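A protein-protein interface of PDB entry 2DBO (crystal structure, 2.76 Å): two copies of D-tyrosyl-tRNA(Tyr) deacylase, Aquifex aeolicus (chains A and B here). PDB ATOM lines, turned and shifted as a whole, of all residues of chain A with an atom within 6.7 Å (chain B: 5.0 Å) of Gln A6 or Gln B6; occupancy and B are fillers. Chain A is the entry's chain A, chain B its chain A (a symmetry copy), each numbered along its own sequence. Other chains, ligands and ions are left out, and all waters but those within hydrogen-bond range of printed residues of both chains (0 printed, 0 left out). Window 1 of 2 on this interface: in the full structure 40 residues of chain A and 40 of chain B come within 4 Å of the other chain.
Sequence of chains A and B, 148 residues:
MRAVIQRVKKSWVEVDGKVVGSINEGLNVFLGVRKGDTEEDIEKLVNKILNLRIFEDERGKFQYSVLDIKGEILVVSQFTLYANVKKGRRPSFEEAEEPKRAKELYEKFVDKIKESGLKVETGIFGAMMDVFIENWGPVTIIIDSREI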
ATOM      1  N   VAL A   4       3.538   1.949   5.266  1.00  0.00           N
ATOM      2  CA  VAL A   4       4.178   0.645   5.185  1.00  0.00           C
ATOM      3  C   VAL A   4       4.638   0.397   6.619  1.00  0.00           C
ATOM      4  O   VAL A   4       5.513   1.097   7.127  1.00  0.00           O
ATOM      5  CB  VAL A   4       5.378   0.630   4.216  1.00  0.00           C
ATOM      6  CG1 VAL A   4       6.142  -0.657   4.388  1.00  0.00           C
ATOM      7  CG2 VAL A   4       4.886   0.727   2.768  1.00  0.00           C
ATOM      8  N   ILE A   5       4.017  -0.567   7.289  1.00  0.00           N
ATOM      9  CA  ILE A   5       4.391  -0.827   8.670  1.00  0.00           C
ATOM     10  C   ILE A   5       5.126  -2.147   8.828  1.00  0.00           C
ATOM     11  O   ILE A   5       4.627  -3.208   8.443  1.00  0.00           O
ATOM     12  CB  ILE A   5       3.156  -0.771   9.620  1.00  0.00           C
ATOM     13  CG1 ILE A   5       3.062  -2.059  10.428  1.00  0.00           C
ATOM     14  CG2 ILE A   5       1.880  -0.487   8.823  1.00  0.00           C
ATOM     15  CD1 ILE A   5       2.065  -2.022  11.558  1.00  0.00           C
ATOM     16  N   GLN A   6       6.326  -2.076   9.390  1.00  0.00           N
ATOM     17  CA  GLN A   6       7.134  -3.270   9.576  1.00  0.00           C
ATOM     18  C   GLN A   6       7.286  -3.645  11.045  1.00  0.00           C
ATOM     19  O   GLN A   6       7.729  -2.828  11.868  1.00  0.00           O
ATOM     20  CB  GLN A   6       8.520  -3.062   8.951  1.00  0.00           C
ATOM     21  CG  GLN A   6       8.491  -2.716   7.458  1.00  0.00           C
ATOM     22  CD  GLN A   6       9.889  -2.553   6.857  1.00  0.00           C
ATOM     23  OE1 GLN A   6      10.607  -3.530   6.631  1.00  0.00           O
ATOM     24  NE2 GLN A   6      10.278  -1.312   6.602  1.00  0.00           N
ATOM     25  N   ARG A   7       6.904  -4.876  11.373  1.00  0.00           N
ATOM     26  CA  ARG A   7       7.024  -5.353  12.746  1.00  0.00           C
ATOM     27  C   ARG A   7       8.517  -5.416  13.032  1.00  0.00           C
ATOM     28  O   ARG A   7       9.267  -6.108  12.329  1.00  0.00           O
ATOM     29  CB  ARG A   7       6.408  -6.750  12.908  1.00  0.00           C
ATOM     30  CG  ARG A   7       6.402  -7.245  14.358  1.00  0.00           C
ATOM     31  CD  ARG A   7       5.758  -8.628  14.522  1.00  0.00           C
ATOM     32  NE  ARG A   7       6.637  -9.716  14.107  1.00  0.00           N
ATOM     33  CZ  ARG A   7       6.313 -11.007  14.160  1.00  0.00           C
ATOM     34  NH1 ARG A   7       5.124 -11.385  14.609  1.00  0.00           N
ATOM     35  NH2 ARG A   7       7.187 -11.926  13.768  1.00  0.00           N
ATOM     36  N   VAL A   8       8.947  -4.693  14.058  1.00  0.00           N
ATOM     37  CA  VAL A   8      10.355  -4.663  14.402  1.00  0.00           C
ATOM     38  C   VAL A   8      10.622  -5.131  15.822  1.00  0.00           C
ATOM     39  O   VAL A   8       9.724  -5.188  16.666  1.00  0.00           O
ATOM     40  CB  VAL A   8      10.933  -3.238  14.254  1.00  0.00           C
ATOM     41  CG1 VAL A   8      10.644  -2.706  12.879  1.00  0.00           C
ATOM     42  CG2 VAL A   8      10.333  -2.322  15.309  1.00  0.00           C
ATOM     43  N   LYS A   9      11.881  -5.446  16.071  1.00  0.00           N
ATOM     44  CA  LYS A   9      12.327  -5.896  17.368  1.00  0.00           C
ATOM     45  C   LYS A   9      13.132  -4.726  17.914  1.00  0.00           C
ATOM     46  O   LYS A   9      13.218  -4.508  19.126  1.00  0.00           O
ATOM     47  CB  LYS A   9      13.207  -7.124  17.175  1.00  0.00           C
ATOM     48  CG  LYS A   9      13.373  -7.977  18.391  1.00  0.00           C
ATOM     49  CD  LYS A   9      13.998  -9.299  18.003  1.00  0.00           C
ATOM     50  CE  LYS A   9      13.067 -10.116  17.132  1.00  0.00           C
ATOM     51  NZ  LYS A   9      13.658 -11.460  16.870  1.00  0.00           N
ATOM     52  N   SER A  11      14.483  -0.637  16.181  1.00  0.00           N
ATOM     53  CA  SER A  11      14.422   0.229  15.017  1.00  0.00           C
ATOM     54  C   SER A  11      14.655   1.690  15.384  1.00  0.00           C
ATOM     55  O   SER A  11      14.080   2.188  16.353  1.00  0.00           O
ATOM     56  CB  SER A  11      13.048   0.061  14.348  1.00  0.00           C
ATOM     57  OG  SER A  11      12.900   0.886  13.210  1.00  0.00           O
ATOM     58  N   GLY A  26       8.287  -3.372  18.688  1.00  0.00           N
ATOM     59  CA  GLY A  26       7.142  -2.565  18.298  1.00  0.00           C
ATOM     60  C   GLY A  26       6.926  -2.437  16.802  1.00  0.00           C
ATOM     61  O   GLY A  26       7.141  -3.384  16.055  1.00  0.00           O
ATOM     62  N   LEU A  27       6.508  -1.254  16.364  1.00  0.00           N
ATOM     63  CA  LEU A  27       6.251  -1.011  14.945  1.00  0.00           C
ATOM     64  C   LEU A  27       6.989   0.168  14.314  1.00  0.00           C
ATOM     65  O   LEU A  27       7.081   1.256  14.894  1.00  0.00           O
ATOM     66  CB  LEU A  27       4.753  -0.780  14.714  1.00  0.00           C
ATOM     67  CG  LEU A  27       3.795  -1.939  14.970  1.00  0.00           C
ATOM     68  CD1 LEU A  27       2.374  -1.426  14.876  1.00  0.00           C
ATOM     69  CD2 LEU A  27       4.054  -3.060  13.964  1.00  0.00           C
ATOM     70  N   ASN A  28       7.517  -0.058  13.117  1.00  0.00           N
ATOM     71  CA  ASN A  28       8.147   1.020  12.379  1.00  0.00           C
ATOM     72  C   ASN A  28       7.066   1.401  11.384  1.00  0.00           C
ATOM     73  O   ASN A  28       6.544   0.540  10.674  1.00  0.00           O
ATOM     74  CB  ASN A  28       9.394   0.551  11.633  1.00  0.00           C
ATOM     75  CG  ASN A  28       9.997   1.655  10.782  1.00  0.00           C
ATOM     76  OD1 ASN A  28       9.555   1.895   9.655  1.00  0.00           O
ATOM     77  ND2 ASN A  28      10.993   2.354  11.327  1.00  0.00           N
ATOM     78  N   VAL A  29       6.710   2.675  11.341  1.00  0.00           N
ATOM     79  CA  VAL A  29       5.669   3.113  10.424  1.00  0.00           C
ATOM     80  C   VAL A  29       6.141   4.128   9.383  1.00  0.00           C
ATOM     81  O   VAL A  29       6.587   5.228   9.721  1.00  0.00           O
ATOM     82  CB  VAL A  29       4.471   3.728  11.195  1.00  0.00           C
ATOM     83  CG1 VAL A  29       3.435   4.282  10.209  1.00  0.00           C
ATOM     84  CG2 VAL A  29       3.837   2.682  12.084  1.00  0.00           C
ATOM     85  N   PHE A  30       6.034   3.745   8.115  1.00  0.00           N
ATOM     86  CA  PHE A  30       6.405   4.611   7.003  1.00  0.00           C
ATOM     87  C   PHE A  30       5.179   5.383   6.596  1.00  0.00           C
ATOM     88  O   PHE A  30       4.191   4.785   6.168  1.00  0.00           O
ATOM     89  CB  PHE A  30       6.846   3.796   5.811  1.00  0.00           C
ATOM     90  CG  PHE A  30       8.288   3.477   5.810  1.00  0.00           C
ATOM     91  CD1 PHE A  30       9.226   4.482   6.024  1.00  0.00           C
ATOM     92  CD2 PHE A  30       8.718   2.178   5.557  1.00  0.00           C
ATOM     93  CE1 PHE A  30      10.578   4.200   5.984  1.00  0.00           C
ATOM     94  CE2 PHE A  30      10.068   1.876   5.511  1.00  0.00           C
ATOM     95  CZ  PHE A  30      11.008   2.889   5.725  1.00  0.00           C
ATOM     96  N   ILE A  54      -0.705  -8.466  14.516  1.00  0.00           N
ATOM     97  CA  ILE A  54       0.416  -9.037  13.765  1.00  0.00           C
ATOM     98  C   ILE A  54       1.437  -9.665  14.703  1.00  0.00           C
ATOM     99  O   ILE A  54       2.263 -10.483  14.280  1.00  0.00           O
ATOM    100  CB  ILE A  54       1.143  -8.002  12.872  1.00  0.00           C
ATOM    101  CG1 ILE A  54       1.579  -6.797  13.703  1.00  0.00           C
ATOM    102  CG2 ILE A  54       0.257  -7.622  11.691  1.00  0.00           C
ATOM    103  CD1 ILE A  54       2.565  -5.891  12.980  1.00  0.00           C
ATOM    104  N   GLN A  78       7.694   9.427   4.632  1.00  0.00           N
ATOM    105  CA  GLN A  78       8.085   8.719   3.419  1.00  0.00           C
ATOM    106  C   GLN A  78       7.180   9.092   2.242  1.00  0.00           C
ATOM    107  O   GLN A  78       6.299   8.317   1.862  1.00  0.00           O
ATOM    108  CB  GLN A  78       8.011   7.202   3.663  1.00  0.00           C
ATOM    109  CG  GLN A  78       8.526   6.353   2.511  1.00  0.00           C
ATOM    110  CD  GLN A  78      10.031   6.448   2.350  1.00  0.00           C
ATOM    111  OE1 GLN A  78      10.757   5.484   2.606  1.00  0.00           O
ATOM    112  NE2 GLN A  78      10.510   7.616   1.929  1.00  0.00           N
ATOM    113  N   VAL A 131      17.488   5.180   8.188  1.00  0.00           N
ATOM    114  CA  VAL A 131      16.540   4.407   8.984  1.00  0.00           C
ATOM    115  C   VAL A 131      16.964   2.963   9.245  1.00  0.00           C
ATOM    116  O   VAL A 131      17.079   2.162   8.318  1.00  0.00           O
ATOM    117  CB  VAL A 131      15.152   4.402   8.304  1.00  0.00           C
ATOM    118  CG1 VAL A 131      14.153   3.652   9.168  1.00  0.00           C
ATOM    119  CG2 VAL A 131      14.685   5.834   8.058  1.00  0.00           C
ATOM    120  N   ILE A 133      16.191  -0.655  10.578  1.00  0.00           N
ATOM    121  CA  ILE A 133      15.071  -1.542  10.843  1.00  0.00           C
ATOM    122  C   ILE A 133      15.451  -2.995  10.988  1.00  0.00           C
ATOM    123  O   ILE A 133      16.142  -3.560  10.146  1.00  0.00           O
ATOM    124  CB  ILE A 133      14.021  -1.463   9.728  1.00  0.00           C
ATOM    125  CG1 ILE A 133      13.551  -0.019   9.552  1.00  0.00           C
ATOM    126  CG2 ILE A 133      12.859  -2.366  10.061  1.00  0.00           C
ATOM    127  CD1 ILE A 133      12.791   0.236   8.259  1.00  0.00           C
ATOM    128  N   GLU A 134      14.970  -3.591  12.068  1.00  0.00           N
ATOM    129  CA  GLU A 134      15.200  -4.987  12.353  1.00  0.00           C
ATOM    130  C   GLU A 134      13.810  -5.613  12.324  1.00  0.00           C
ATOM    131  O   GLU A 134      13.115  -5.692  13.340  1.00  0.00           O
ATOM    132  CB  GLU A 134      15.841  -5.127  13.725  1.00  0.00           C
ATOM    133  CG  GLU A 134      16.750  -6.315  13.822  1.00  0.00           C
ATOM    134  CD  GLU A 134      17.582  -6.313  15.087  1.00  0.00           C
ATOM    135  OE1 GLU A 134      18.394  -5.367  15.286  1.00  0.00           O
ATOM    136  OE2 GLU A 134      17.416  -7.274  15.871  1.00  0.00           O
ATOM    137  N   ASN A 135      13.411  -6.028  11.129  1.00  0.00           N
ATOM    138  CA  ASN A 135      12.107  -6.620  10.891  1.00  0.00           C
ATOM    139  C   ASN A 135      12.078  -8.089  11.311  1.00  0.00           C
ATOM    140  O   ASN A 135      12.690  -8.951  10.675  1.00  0.00           O
ATOM    141  CB  ASN A 135      11.757  -6.471   9.410  1.00  0.00           C
ATOM    142  CG  ASN A 135      10.327  -6.856   9.102  1.00  0.00           C
ATOM    143  OD1 ASN A 135       9.675  -7.554   9.881  1.00  0.00           O
ATOM    144  ND2 ASN A 135       9.834  -6.420   7.948  1.00  0.00           N
ATOM    145  N   TRP A 136      11.355  -8.354  12.394  1.00  0.00           N
ATOM    146  CA  TRP A 136      11.212  -9.689  12.953  1.00  0.00           C
ATOM    147  C   TRP A 136      10.127 -10.472  12.221  1.00  0.00           C
ATOM    148  O   TRP A 136       8.950 -10.095  12.238  1.00  0.00           O
ATOM    149  CB  TRP A 136      10.883  -9.556  14.445  1.00  0.00           C
ATOM    150  CG  TRP A 136      10.385 -10.792  15.159  1.00  0.00           C
ATOM    151  CD1 TRP A 136      10.744 -12.097  14.930  1.00  0.00           C
ATOM    152  CD2 TRP A 136       9.507 -10.810  16.295  1.00  0.00           C
ATOM    153  NE1 TRP A 136      10.148 -12.921  15.863  1.00  0.00           N
ATOM    154  CE2 TRP A 136       9.393 -12.159  16.712  1.00  0.00           C
ATOM    155  CE3 TRP A 136       8.826  -9.813  17.012  1.00  0.00           C
ATOM    156  CZ2 TRP A 136       8.605 -12.533  17.809  1.00  0.00           C
ATOM    157  CZ3 TRP A 136       8.046 -10.187  18.104  1.00  0.00           C
ATOM    158  CH2 TRP A 136       7.948 -11.536  18.495  1.00  0.00           C
ATOM    159  N   PRO A 138      10.132 -11.786   8.537  1.00  0.00           N
ATOM    160  CA  PRO A 138       9.744 -10.387   8.748  1.00  0.00           C
ATOM    161  C   PRO A 138       8.242 -10.209   8.516  1.00  0.00           C
ATOM    162  O   PRO A 138       7.610 -11.027   7.844  1.00  0.00           O
ATOM    163  CB  PRO A 138      10.578  -9.652   7.706  1.00  0.00           C
ATOM    164  CG  PRO A 138      10.521 -10.597   6.561  1.00  0.00           C
ATOM    165  CD  PRO A 138      10.786 -11.945   7.226  1.00  0.00           C
ATOM    166  N   VAL A 139       7.670  -9.147   9.073  1.00  0.00           N
ATOM    167  CA  VAL A 139       6.242  -8.877   8.907  1.00  0.00           C
ATOM    168  C   VAL A 139       6.052  -7.457   8.413  1.00  0.00           C
ATOM    169  O   VAL A 139       6.371  -6.494   9.113  1.00  0.00           O
ATOM    170  CB  VAL A 139       5.454  -9.017  10.228  1.00  0.00           C
ATOM    171  CG1 VAL A 139       3.993  -8.658   9.975  1.00  0.00           C
ATOM    172  CG2 VAL A 139       5.582 -10.444  10.788  1.00  0.00           C
ATOM    173  N   THR A 140       5.512  -7.335   7.212  1.00  0.00           N
ATOM    174  CA  THR A 140       5.298  -6.029   6.613  1.00  0.00           C
ATOM    175  C   THR A 140       3.884  -5.914   6.081  1.00  0.00           C
ATOM    176  O   THR A 140       3.412  -6.796   5.364  1.00  0.00           O
ATOM    177  CB  THR A 140       6.283  -5.820   5.459  1.00  0.00           C
ATOM    178  OG1 THR A 140       7.598  -6.217   5.886  1.00  0.00           O
ATOM    179  CG2 THR A 140       6.280  -4.350   5.025  1.00  0.00           C
ATOM    180  N   ILE A 141       3.211  -4.828   6.431  1.00  0.00           N
ATOM    181  CA  ILE A 141       1.834  -4.635   5.984  1.00  0.00           C
ATOM    182  C   ILE A 141       1.675  -3.278   5.306  1.00  0.00           C
ATOM    183  O   ILE A 141       2.295  -2.291   5.723  1.00  0.00           O
ATOM    184  CB  ILE A 141       0.834  -4.708   7.184  1.00  0.00           C
ATOM    185  CG1 ILE A 141       1.069  -5.972   8.026  1.00  0.00           C
ATOM    186  CG2 ILE A 141      -0.596  -4.669   6.662  1.00  0.00           C
ATOM    187  CD1 ILE A 141       0.896  -7.302   7.284  1.00  0.00           C
ATOM    188  N   VAL B   4       7.849  -4.737  -1.960  1.00  0.00           N
ATOM    189  CA  VAL B   4       8.164  -3.518  -1.231  1.00  0.00           C
ATOM    190  C   VAL B   4       9.686  -3.448  -1.317  1.00  0.00           C
ATOM    191  O   VAL B   4      10.387  -4.290  -0.755  1.00  0.00           O
ATOM    192  CB  VAL B   4       7.703  -3.570   0.240  1.00  0.00           C
ATOM    193  CG1 VAL B   4       8.294  -2.404   0.989  1.00  0.00           C
ATOM    194  CG2 VAL B   4       6.175  -3.486   0.316  1.00  0.00           C
ATOM    195  N   ILE B   5      10.200  -2.475  -2.060  1.00  0.00           N
ATOM    196  CA  ILE B   5      11.643  -2.377  -2.206  1.00  0.00           C
ATOM    197  C   ILE B   5      12.215  -1.174  -1.477  1.00  0.00           C
ATOM    198  O   ILE B   5      11.808  -0.032  -1.706  1.00  0.00           O
ATOM    199  CB  ILE B   5      12.069  -2.361  -3.707  1.00  0.00           C
ATOM    200  CG1 ILE B   5      12.939  -1.143  -3.987  1.00  0.00           C
ATOM    201  CG2 ILE B   5      10.837  -2.420  -4.614  1.00  0.00           C
ATOM    202  CD1 ILE B   5      13.620  -1.151  -5.331  1.00  0.00           C
ATOM    203  N   GLN B   6      13.159  -1.438  -0.581  1.00  0.00           N
ATOM    204  CA  GLN B   6      13.768  -0.371   0.196  1.00  0.00           C
ATOM    205  C   GLN B   6      15.227  -0.140  -0.180  1.00  0.00           C
ATOM    206  O   GLN B   6      16.049  -1.070  -0.143  1.00  0.00           O
ATOM    207  CB  GLN B   6      13.665  -0.693   1.693  1.00  0.00           C
ATOM    208  CG  GLN B   6      12.232  -0.908   2.191  1.00  0.00           C
ATOM    209  CD  GLN B   6      12.160  -1.190   3.695  1.00  0.00           C
ATOM    210  OE1 GLN B   6      12.330  -0.293   4.523  1.00  0.00           O
ATOM    211  NE2 GLN B   6      11.914  -2.444   4.045  1.00  0.00           N
ATOM    212  N   ARG B   7      15.542   1.097  -0.553  1.00  0.00           N
ATOM    213  CA  ARG B   7      16.913   1.441  -0.912  1.00  0.00           C
ATOM    214  C   ARG B   7      17.724   1.298   0.367  1.00  0.00           C
ATOM    215  O   ARG B   7      17.429   1.949   1.379  1.00  0.00           O
ATOM    216  CB  ARG B   7      17.011   2.884  -1.426  1.00  0.00           C
ATOM    217  CG  ARG B   7      18.411   3.255  -1.930  1.00  0.00           C
ATOM    218  CD  ARG B   7      18.498   4.687  -2.472  1.00  0.00           C
ATOM    219  NE  ARG B   7      18.564   5.690  -1.415  1.00  0.00           N
ATOM    220  CZ  ARG B   7      18.653   7.003  -1.627  1.00  0.00           C
ATOM    221  NH1 ARG B   7      18.685   7.484  -2.863  1.00  0.00           N
ATOM    222  NH2 ARG B   7      18.718   7.837  -0.596  1.00  0.00           N
ATOM    223  N   VAL B   8      18.740   0.445   0.324  1.00  0.00           N
ATOM    224  CA  VAL B   8      19.562   0.215   1.496  1.00  0.00           C
ATOM    225  C   VAL B   8      21.029   0.528   1.253  1.00  0.00           C
ATOM    226  O   VAL B   8      21.491   0.623   0.114  1.00  0.00           O
ATOM    227  CB  VAL B   8      19.460  -1.253   1.967  1.00  0.00           C
ATOM    228  CG1 VAL B   8      18.020  -1.630   2.166  1.00  0.00           C
ATOM    229  CG2 VAL B   8      20.107  -2.173   0.944  1.00  0.00           C
ATOM    230  N   GLY B  26      22.621  -1.165  -2.118  1.00  0.00           N
ATOM    231  CA  GLY B  26      21.750  -1.791  -3.098  1.00  0.00           C
ATOM    232  C   GLY B  26      20.273  -1.767  -2.752  1.00  0.00           C
ATOM    233  O   GLY B  26      19.775  -0.796  -2.197  1.00  0.00           O
ATOM    234  N   LEU B  27      19.573  -2.851  -3.073  1.00  0.00           N
ATOM    235  CA  LEU B  27      18.139  -2.942  -2.804  1.00  0.00           C
ATOM    236  C   LEU B  27      17.678  -4.146  -1.985  1.00  0.00           C
ATOM    237  O   LEU B  27      18.114  -5.282  -2.204  1.00  0.00           O
ATOM    238  CB  LEU B  27      17.356  -2.969  -4.122  1.00  0.00           C
ATOM    239  CG  LEU B  27      17.388  -1.726  -5.008  1.00  0.00           C
ATOM    240  CD1 LEU B  27      16.726  -2.053  -6.329  1.00  0.00           C
ATOM    241  CD2 LEU B  27      16.688  -0.567  -4.301  1.00  0.00           C
ATOM    242  N   ASN B  28      16.788  -3.887  -1.033  1.00  0.00           N
ATOM    243  CA  ASN B  28      16.202  -4.970  -0.265  1.00  0.00           C
ATOM    244  C   ASN B  28      14.846  -5.132  -0.926  1.00  0.00           C
ATOM    245  O   ASN B  28      14.106  -4.158  -1.074  1.00  0.00           O
ATOM    246  CB  ASN B  28      16.019  -4.595   1.204  1.00  0.00           C
ATOM    247  CG  ASN B  28      15.316  -5.690   1.987  1.00  0.00           C
ATOM    248  OD1 ASN B  28      14.086  -5.780   1.977  1.00  0.00           O
ATOM    249  ND2 ASN B  28      16.093  -6.548   2.647  1.00  0.00           N
ATOM    250  N   PHE B  30      11.165  -7.053  -0.860  1.00  0.00           N
ATOM    251  CA  PHE B  30      10.165  -7.863  -0.176  1.00  0.00           C
ATOM    252  C   PHE B  30       9.253  -8.444  -1.221  1.00  0.00           C
ATOM    253  O   PHE B  30       8.573  -7.696  -1.927  1.00  0.00           O
ATOM    254  CB  PHE B  30       9.321  -7.012   0.743  1.00  0.00           C
ATOM    255  CG  PHE B  30       9.880  -6.872   2.103  1.00  0.00           C
ATOM    256  CD1 PHE B  30      10.293  -7.999   2.808  1.00  0.00           C
ATOM    257  CD2 PHE B  30       9.959  -5.619   2.703  1.00  0.00           C
ATOM    258  CE1 PHE B  30      10.778  -7.881   4.097  1.00  0.00           C
ATOM    259  CE2 PHE B  30      10.441  -5.481   3.993  1.00  0.00           C
ATOM    260  CZ  PHE B  30      10.853  -6.615   4.699  1.00  0.00           C
ATOM    261  N   ILE B 133      17.643  -4.144   7.981  1.00  0.00           N
ATOM    262  CA  ILE B 133      17.592  -3.153   6.921  1.00  0.00           C
ATOM    263  C   ILE B 133      18.041  -1.773   7.338  1.00  0.00           C
ATOM    264  O   ILE B 133      17.581  -1.229   8.337  1.00  0.00           O
ATOM    265  CB  ILE B 133      16.173  -3.010   6.358  1.00  0.00           C
ATOM    266  CG1 ILE B 133      15.664  -4.366   5.868  1.00  0.00           C
ATOM    267  CG2 ILE B 133      16.172  -2.002   5.234  1.00  0.00           C
ATOM    268  CD1 ILE B 133      14.164  -4.418   5.626  1.00  0.00           C
ATOM    269  N   ASN B 135      17.804   1.464   5.651  1.00  0.00           N
ATOM    270  CA  ASN B 135      17.187   2.228   4.582  1.00  0.00           C
ATOM    271  C   ASN B 135      17.743   3.649   4.521  1.00  0.00           C
ATOM    272  O   ASN B 135      17.481   4.481   5.394  1.00  0.00           O
ATOM    273  CB  ASN B 135      15.673   2.246   4.797  1.00  0.00           C
ATOM    274  CG  ASN B 135      14.919   2.827   3.621  1.00  0.00           C
ATOM    275  OD1 ASN B 135      15.489   3.531   2.787  1.00  0.00           O
ATOM    276  ND2 ASN B 135      13.621   2.551   3.558  1.00  0.00           N
ATOM    277  N   VAL B 139      14.213   5.419   1.365  1.00  0.00           N
ATOM    278  CA  VAL B 139      13.511   5.339   0.084  1.00  0.00           C
ATOM    279  C   VAL B 139      12.813   3.999  -0.025  1.00  0.00           C
ATOM    280  O   VAL B 139      13.458   2.950  -0.071  1.00  0.00           O
ATOM    281  CB  VAL B 139      14.465   5.464  -1.125  1.00  0.00           C
ATOM    282  CG1 VAL B 139      13.660   5.309  -2.411  1.00  0.00           C
ATOM    283  CG2 VAL B 139      15.203   6.813  -1.095  1.00  0.00           C
ATOM    284  N   THR B 140      11.492   4.043  -0.088  1.00  0.00           N
ATOM    285  CA  THR B 140      10.702   2.828  -0.172  1.00  0.00           C
ATOM    286  C   THR B 140       9.686   2.930  -1.292  1.00  0.00           C
ATOM    287  O   THR B 140       8.960   3.920  -1.388  1.00  0.00           O
ATOM    288  CB  THR B 140       9.965   2.596   1.150  1.00  0.00           C
ATOM    289  OG1 THR B 140      10.883   2.794   2.239  1.00  0.00           O
ATOM    290  CG2 THR B 140       9.383   1.179   1.187  1.00  0.00           C
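O of Val A131 lies close to O of Ile B133 (3.4 Å). OE1 of Gln A6 sits at hydrogen-bond distance from NE2 of Gln B6, 3.1 Å away. O of Val A131 lies within hydrogen-bond range of N of Asn B135, 2.9 Å away. The side-chain hydroxyl (OG1) of Thr B140 lies within hydrogen-bond range of the side-chain amide oxygen (OE1) of Gln A78. N of Ile A133 is in hydrogen-bond range of O of Ile B133 (2.7 Å).
The side-chain amide oxygen of Gln B6 sits at hydrogen-bond distance from the side-chain amide nitrogen of Asn B135 (3.3 Å). The side-chain amide oxygen (OD1) of Asn B135 lies within hydrogen-bond range of the backbone NH (N) of Val B139 (2.7 Å). The side-chain hydroxyl (OG1) of Thr B140 lies within hydrogen-bond range of the side-chain amide nitrogen (ND2) of Asn B135, 3.0 Å away. N of Phe A30 is in hydrogen-bond range of O of Val A4. The backbone carbonyl oxygen (O) of Arg B7 lies close to the side-chain amide oxygen (OD1) of Asn B135 (2.9 Å). OG1 of Thr A140 lies within hydrogen-bond range of ND2 of Asn A135 (3.0 Å).
Among the printed residues, merely in contact across the chains: Gln A6 with Phe B30 (3.3 Å), Phe A30 with Gln B6 (3.3 Å), Asn A135 with Phe B30 (3.4 Å), Phe A30 with Asn B135 (3.4 Å), Thr A140 with Phe B30 (3.5 Å), Phe A30 with Thr B140 (3.5 Å), Gln A78 with Val B139 (3.7 Å), Pro A138 with Phe B30 (3.7 Å), Ile A133 with Gln B6 (3.8 Å) and Gln A6 with Ile B133 (3.8 Å).
Of chain B, only Gln B6 (3.1 Å), Phe B30 (3.3 Å) and Ile B133 (3.8 Å) come within 4 Å of Gln A6. Printed residues of chain B within 4 Å of Pro A138: Phe B30 (3.7 Å). Of the printed residues of chain A, Val B139 touches Gln A78. The nearest printed residue of chain B that does not touch Gln A6 is Asn B135 (5.9 Å). The nearest printed residue of chain B that does not touch Thr A140 is Val B4 (4.8 Å).
Of the 13 printed residues of chain B, 6 touch a printed residue of chain A. Printed residues of chain A that touch a printed residue of chain B: Gln A6, Phe A30, Gln A78, Val A131, Ile A133, Asn A135, Pro A138 and Thr A140. Hydrophobic or aromatic side chains of chain A that line the printed part of chain B: Phe A30, Val A131, Ile A133 and Pro A138.
Gln A6 touches Phe B30, and with the chains exchanged Phe A30 touches Gln B6. Gln A6 touches Ile B133, and with the chains exchanged Ile A133 touches Gln B6. Phe A30 touches Thr B140, and with the chains exchanged Thr A140 touches Phe B30. Ile B133 touches its own counterpart, Ile A133.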
